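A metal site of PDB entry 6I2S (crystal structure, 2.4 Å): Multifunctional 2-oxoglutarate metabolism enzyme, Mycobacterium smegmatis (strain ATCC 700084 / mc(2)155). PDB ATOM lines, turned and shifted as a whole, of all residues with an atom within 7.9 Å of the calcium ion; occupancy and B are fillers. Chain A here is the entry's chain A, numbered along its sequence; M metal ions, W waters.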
ATOM      1  N   LYS A 535      10.663  -9.501  -6.724  1.00  0.00           N
ATOM      2  CA  LYS A 535       9.569  -8.652  -7.173  1.00  0.00           C
ATOM      3  C   LYS A 535       8.210  -9.332  -7.111  1.00  0.00           C
ATOM      4  O   LYS A 535       8.082 -10.506  -7.486  1.00  0.00           O
ATOM      5  CB  LYS A 535       9.821  -8.175  -8.612  1.00  0.00           C
ATOM      6  CG  LYS A 535       9.157  -6.843  -8.935  1.00  0.00           C
ATOM      7  CD  LYS A 535       9.368  -6.471 -10.378  1.00  0.00           C
ATOM      8  CE  LYS A 535       8.774  -5.122 -10.703  1.00  0.00           C
ATOM      9  NZ  LYS A 535       9.489  -4.003 -10.046  1.00  0.00           N
ATOM     10  N   PRO A 608       4.141   0.818  -6.524  1.00  0.00           N
ATOM     11  CA  PRO A 608       5.013   1.066  -7.682  1.00  0.00           C
ATOM     12  C   PRO A 608       6.094  -0.008  -7.902  1.00  0.00           C
ATOM     13  O   PRO A 608       6.655  -0.073  -8.994  1.00  0.00           O
ATOM     14  CB  PRO A 608       5.672   2.416  -7.360  1.00  0.00           C
ATOM     15  CG  PRO A 608       4.770   3.040  -6.348  1.00  0.00           C
ATOM     16  CD  PRO A 608       4.266   1.897  -5.526  1.00  0.00           C
ATOM     17  N   ALA A 610       5.560  -3.294  -7.712  1.00  0.00           N
ATOM     18  CA  ALA A 610       4.929  -4.479  -8.271  1.00  0.00           C
ATOM     19  C   ALA A 610       4.972  -4.432  -9.783  1.00  0.00           C
ATOM     20  O   ALA A 610       4.967  -3.348 -10.359  1.00  0.00           O
ATOM     21  CB  ALA A 610       3.492  -4.571  -7.781  1.00  0.00           C
ATOM     22  N   MET A 611       5.052  -5.596 -10.427  1.00  0.00           N
ATOM     23  CA  MET A 611       4.977  -5.787 -11.877  1.00  0.00           C
ATOM     24  C   MET A 611       3.518  -6.137 -12.124  1.00  0.00           C
ATOM     25  O   MET A 611       3.070  -7.195 -11.682  1.00  0.00           O
ATOM     26  CB  MET A 611       5.970  -6.887 -12.318  1.00  0.00           C
ATOM     27  CG  MET A 611       5.912  -7.216 -13.795  1.00  0.00           C
ATOM     28  SD  MET A 611       6.966  -6.197 -14.861  1.00  0.00           S
ATOM     29  CE  MET A 611       6.718  -7.001 -16.389  1.00  0.00           C
ATOM     30  N   SER A 644       2.103   5.315 -13.010  1.00  0.00           N
ATOM     31  CA  SER A 644       1.678   3.924 -13.101  1.00  0.00           C
ATOM     32  C   SER A 644       2.634   3.144 -13.986  1.00  0.00           C
ATOM     33  O   SER A 644       3.074   3.653 -15.013  1.00  0.00           O
ATOM     34  CB  SER A 644       0.264   3.845 -13.644  1.00  0.00           C
ATOM     35  OG  SER A 644      -0.109   2.536 -14.034  1.00  0.00           O
ATOM     36  N   ASP A 645       2.921   1.914 -13.604  1.00  0.00           N
ATOM     37  CA  ASP A 645       3.811   1.027 -14.358  1.00  0.00           C
ATOM     38  C   ASP A 645       3.013  -0.154 -14.877  1.00  0.00           C
ATOM     39  O   ASP A 645       3.559  -1.257 -15.002  1.00  0.00           O
ATOM     40  CB  ASP A 645       4.976   0.565 -13.451  1.00  0.00           C
ATOM     41  CG  ASP A 645       6.268   0.212 -14.164  1.00  0.00           C
ATOM     42  OD1 ASP A 645       6.668   0.974 -15.071  1.00  0.00           O
ATOM     43  OD2 ASP A 645       6.872  -0.824 -13.803  1.00  0.00           O
ATOM     44  N   VAL A 646       1.708   0.054 -15.164  1.00  0.00           N
ATOM     45  CA  VAL A 646       0.828  -1.042 -15.599  1.00  0.00           C
ATOM     46  C   VAL A 646       1.190  -1.520 -17.019  1.00  0.00           C
ATOM     47  O   VAL A 646       1.493  -0.712 -17.903  1.00  0.00           O
ATOM     48  CB  VAL A 646      -0.700  -0.720 -15.441  1.00  0.00           C
ATOM     49  CG1 VAL A 646      -1.187   0.357 -16.407  1.00  0.00           C
ATOM     50  CG2 VAL A 646      -1.569  -1.979 -15.547  1.00  0.00           C
ATOM     51  N   VAL A 647       1.153  -2.842 -17.231  1.00  0.00           N
ATOM     52  CA  VAL A 647       1.373  -3.475 -18.527  1.00  0.00           C
ATOM     53  C   VAL A 647       0.029  -3.952 -19.050  1.00  0.00           C
ATOM     54  O   VAL A 647      -0.715  -4.596 -18.320  1.00  0.00           O
ATOM     55  CB  VAL A 647       2.403  -4.644 -18.510  1.00  0.00           C
ATOM     56  CG1 VAL A 647       2.668  -5.202 -19.914  1.00  0.00           C
ATOM     57  CG2 VAL A 647       3.703  -4.236 -17.833  1.00  0.00           C
ATOM     58  N   LEU A 693       9.867  -7.129 -21.030  1.00  0.00           N
ATOM     59  CA  LEU A 693       9.230  -7.268 -19.708  1.00  0.00           C
ATOM     60  C   LEU A 693      10.227  -7.030 -18.554  1.00  0.00           C
ATOM     61  O   LEU A 693       9.889  -6.341 -17.593  1.00  0.00           O
ATOM     62  CB  LEU A 693       8.557  -8.647 -19.527  1.00  0.00           C
ATOM     63  CG  LEU A 693       7.317  -8.990 -20.377  1.00  0.00           C
ATOM     64  CD1 LEU A 693       6.814 -10.395 -20.058  1.00  0.00           C
ATOM     65  CD2 LEU A 693       6.194  -7.988 -20.159  1.00  0.00           C
ATOM     66  N   ARG A 694      11.418  -7.617 -18.646  1.00  0.00           N
ATOM     67  CA  ARG A 694      12.458  -7.515 -17.609  1.00  0.00           C
ATOM     68  C   ARG A 694      12.931  -6.071 -17.449  1.00  0.00           C
ATOM     69  O   ARG A 694      13.139  -5.624 -16.322  1.00  0.00           O
ATOM     70  CB  ARG A 694      13.651  -8.426 -17.933  1.00  0.00           C
ATOM     71  CG  ARG A 694      13.329  -9.916 -18.011  1.00  0.00           C
ATOM     72  CD  ARG A 694      13.789 -10.717 -16.815  1.00  0.00           C
ATOM     73  NE  ARG A 694      15.165 -10.401 -16.444  1.00  0.00           N
ATOM     74  CZ  ARG A 694      15.619 -10.438 -15.198  1.00  0.00           C
ATOM     75  NH1 ARG A 694      14.827 -10.801 -14.199  1.00  0.00           N
ATOM     76  NH2 ARG A 694      16.887 -10.109 -14.946  1.00  0.00           N
ATOM     77  N   ARG A 695      13.070  -5.342 -18.576  1.00  0.00           N
ATOM     78  CA  ARG A 695      13.473  -3.931 -18.566  1.00  0.00           C
ATOM     79  C   ARG A 695      12.372  -3.123 -17.910  1.00  0.00           C
ATOM     80  O   ARG A 695      12.667  -2.298 -17.046  1.00  0.00           O
ATOM     81  CB  ARG A 695      13.766  -3.440 -19.990  1.00  0.00           C
ATOM     82  CG  ARG A 695      14.144  -1.970 -20.086  1.00  0.00           C
ATOM     83  CD  ARG A 695      14.293  -1.547 -21.531  1.00  0.00           C
ATOM     84  NE  ARG A 695      13.019  -1.374 -22.237  1.00  0.00           N
ATOM     85  CZ  ARG A 695      12.879  -0.694 -23.366  1.00  0.00           C
ATOM     86  NH1 ARG A 695      13.931  -0.102 -23.919  1.00  0.00           N
ATOM     87  NH2 ARG A 695      11.689  -0.585 -23.943  1.00  0.00           N
ATOM     88  N   HIS A 696      11.110  -3.401 -18.289  1.00  0.00           N
ATOM     89  CA  HIS A 696       9.942  -2.724 -17.745  1.00  0.00           C
ATOM     90  C   HIS A 696       9.900  -2.841 -16.209  1.00  0.00           C
ATOM     91  O   HIS A 696       9.633  -1.834 -15.540  1.00  0.00           O
ATOM     92  CB  HIS A 696       8.659  -3.261 -18.373  1.00  0.00           C
ATOM     93  CG  HIS A 696       7.450  -2.567 -17.843  1.00  0.00           C
ATOM     94  ND1 HIS A 696       7.135  -1.281 -18.250  1.00  0.00           N
ATOM     95  CD2 HIS A 696       6.592  -2.935 -16.876  1.00  0.00           C
ATOM     96  CE1 HIS A 696       6.061  -0.932 -17.544  1.00  0.00           C
ATOM     97  NE2 HIS A 696       5.707  -1.900 -16.701  1.00  0.00           N
ATOM     98  N   GLY A 697      10.174  -4.026 -15.673  1.00  0.00           N
ATOM     99  CA  GLY A 697      10.147  -4.281 -14.237  1.00  0.00           C
ATOM    100  C   GLY A 697      11.389  -3.893 -13.463  1.00  0.00           C
ATOM    101  O   GLY A 697      11.352  -3.884 -12.231  1.00  0.00           O
ATOM    102  N   LYS A 698      12.502  -3.556 -14.147  1.00  0.00           N
ATOM    103  CA  LYS A 698      13.750  -3.237 -13.460  1.00  0.00           C
ATOM    104  C   LYS A 698      14.312  -1.838 -13.786  1.00  0.00           C
ATOM    105  O   LYS A 698      15.319  -1.464 -13.171  1.00  0.00           O
ATOM    106  CB  LYS A 698      14.823  -4.296 -13.807  1.00  0.00           C
ATOM    107  CG  LYS A 698      14.511  -5.732 -13.390  1.00  0.00           C
ATOM    108  CD  LYS A 698      15.584  -6.713 -13.886  1.00  0.00           C
ATOM    109  CE  LYS A 698      16.934  -6.614 -13.175  1.00  0.00           C
ATOM    110  NZ  LYS A 698      16.855  -7.058 -11.751  1.00  0.00           N
ATOM    111  N   ASP A 699      13.717  -1.082 -14.724  1.00  0.00           N
ATOM    112  CA  ASP A 699      14.240   0.221 -15.148  1.00  0.00           C
ATOM    113  C   ASP A 699      14.139   1.347 -14.084  1.00  0.00           C
ATOM    114  O   ASP A 699      14.716   2.414 -14.293  1.00  0.00           O
ATOM    115  CB  ASP A 699      13.594   0.704 -16.483  1.00  0.00           C
ATOM    116  CG  ASP A 699      12.077   0.791 -16.563  1.00  0.00           C
ATOM    117  OD1 ASP A 699      11.410   0.712 -15.494  1.00  0.00           O
ATOM    118  OD2 ASP A 699      11.549   0.946 -17.686  1.00  0.00           O
ATOM    119  N   GLY A 700      13.427   1.121 -12.987  1.00  0.00           N
ATOM    120  CA  GLY A 700      13.250   2.132 -11.949  1.00  0.00           C
ATOM    121  C   GLY A 700      12.476   3.355 -12.411  1.00  0.00           C
ATOM    122  O   GLY A 700      12.611   4.432 -11.821  1.00  0.00           O
ATOM    123  N   ILE A 701      11.686   3.204 -13.493  1.00  0.00           N
ATOM    124  CA  ILE A 701      10.818   4.216 -14.102  1.00  0.00           C
ATOM    125  C   ILE A 701       9.402   3.696 -14.010  1.00  0.00           C
ATOM    126  O   ILE A 701       9.189   2.502 -14.243  1.00  0.00           O
ATOM    127  CB  ILE A 701      11.256   4.542 -15.580  1.00  0.00           C
ATOM    128  CG1 ILE A 701      12.600   5.325 -15.604  1.00  0.00           C
ATOM    129  CG2 ILE A 701      10.155   5.277 -16.393  1.00  0.00           C
ATOM    130  CD1 ILE A 701      13.156   5.588 -17.038  1.00  0.00           C
ATOM    131  N   GLN A 702       8.446   4.559 -13.641  1.00  0.00           N
ATOM    132  CA  GLN A 702       7.021   4.199 -13.591  1.00  0.00           C
ATOM    133  C   GLN A 702       6.380   4.729 -14.870  1.00  0.00           C
ATOM    134  O   GLN A 702       6.108   5.938 -14.963  1.00  0.00           O
ATOM    135  CB  GLN A 702       6.305   4.743 -12.325  1.00  0.00           C
ATOM    136  CG  GLN A 702       6.923   4.349 -10.983  1.00  0.00           C
ATOM    137  CD  GLN A 702       7.124   2.857 -10.854  1.00  0.00           C
ATOM    138  OE1 GLN A 702       6.168   2.107 -10.695  1.00  0.00           O
ATOM    139  NE2 GLN A 702       8.385   2.408 -10.927  1.00  0.00           N
ATOM    140  N   ARG A 703       6.201   3.854 -15.871  1.00  0.00           N
ATOM    141  CA  ARG A 703       5.598   4.255 -17.153  1.00  0.00           C
ATOM    142  C   ARG A 703       4.786   3.090 -17.733  1.00  0.00           C
ATOM    143  O   ARG A 703       5.308   1.974 -17.800  1.00  0.00           O
ATOM    144  CB  ARG A 703       6.677   4.731 -18.141  1.00  0.00           C
ATOM    145  CG  ARG A 703       6.117   5.352 -19.416  1.00  0.00           C
ATOM    146  CD  ARG A 703       7.195   6.050 -20.222  1.00  0.00           C
ATOM    147  NE  ARG A 703       7.740   7.195 -19.489  1.00  0.00           N
ATOM    148  CZ  ARG A 703       8.955   7.693 -19.686  1.00  0.00           C
ATOM    149  NH1 ARG A 703       9.758   7.165 -20.594  1.00  0.00           N
ATOM    150  NH2 ARG A 703       9.364   8.728 -18.971  1.00  0.00           N
ATOM    151  N   PRO A 704       3.510   3.316 -18.128  1.00  0.00           N
ATOM    152  CA  PRO A 704       2.705   2.199 -18.650  1.00  0.00           C
ATOM    153  C   PRO A 704       3.312   1.594 -19.901  1.00  0.00           C
ATOM    154  O   PRO A 704       3.980   2.279 -20.679  1.00  0.00           O
ATOM    155  CB  PRO A 704       1.344   2.840 -18.926  1.00  0.00           C
ATOM    156  CG  PRO A 704       1.308   4.066 -18.070  1.00  0.00           C
ATOM    157  CD  PRO A 704       2.718   4.564 -18.093  1.00  0.00           C
ATOM    158  N   LEU A 705       3.137   0.275 -20.048  1.00  0.00           N
ATOM    159  CA  LEU A 705       3.650  -0.471 -21.182  1.00  0.00           C
ATOM    160  C   LEU A 705       2.469  -1.151 -21.935  1.00  0.00           C
ATOM    161  O   LEU A 705       1.745  -1.968 -21.360  1.00  0.00           O
ATOM    162  CB  LEU A 705       4.722  -1.507 -20.733  1.00  0.00           C
ATOM    163  CG  LEU A 705       5.159  -2.579 -21.769  1.00  0.00           C
ATOM    164  CD1 LEU A 705       5.878  -1.980 -22.960  1.00  0.00           C
ATOM    165  CD2 LEU A 705       6.000  -3.659 -21.133  1.00  0.00           C
HETATM  166 CA    CA M   1       9.039   0.212 -14.898  1.00  0.00          CA
HETATM  167  O   HOH W   1       9.920   0.047 -12.549  1.00  0.00           O
HETATM  168  O   HOH W   2       8.934   1.115 -17.215  1.00  0.00           O
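OD1 of Asp 645 sits close to N of Arg 703, 3.0 Å away.
Four residues have an atom within 4 Å of the calcium ion: Asp 645, His 696, Asp 699 and Ile 701.
Water W2 bridges the side-chain carboxylate of Asp 699 (2.7 Å) and a ring nitrogen (ND1) of His 696 (3.2 Å).
The calcium ion is bound by the backbone carbonyl oxygen (O) of His 696, the backbone carbonyl oxygen (O) of Ile 701, water W2, the side-chain carboxylate (OD1) of Asp 699, the side-chain carboxylate (OD1) of Asp 645, water W1 and the side-chain carboxylate (OD2) of Asp 645.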
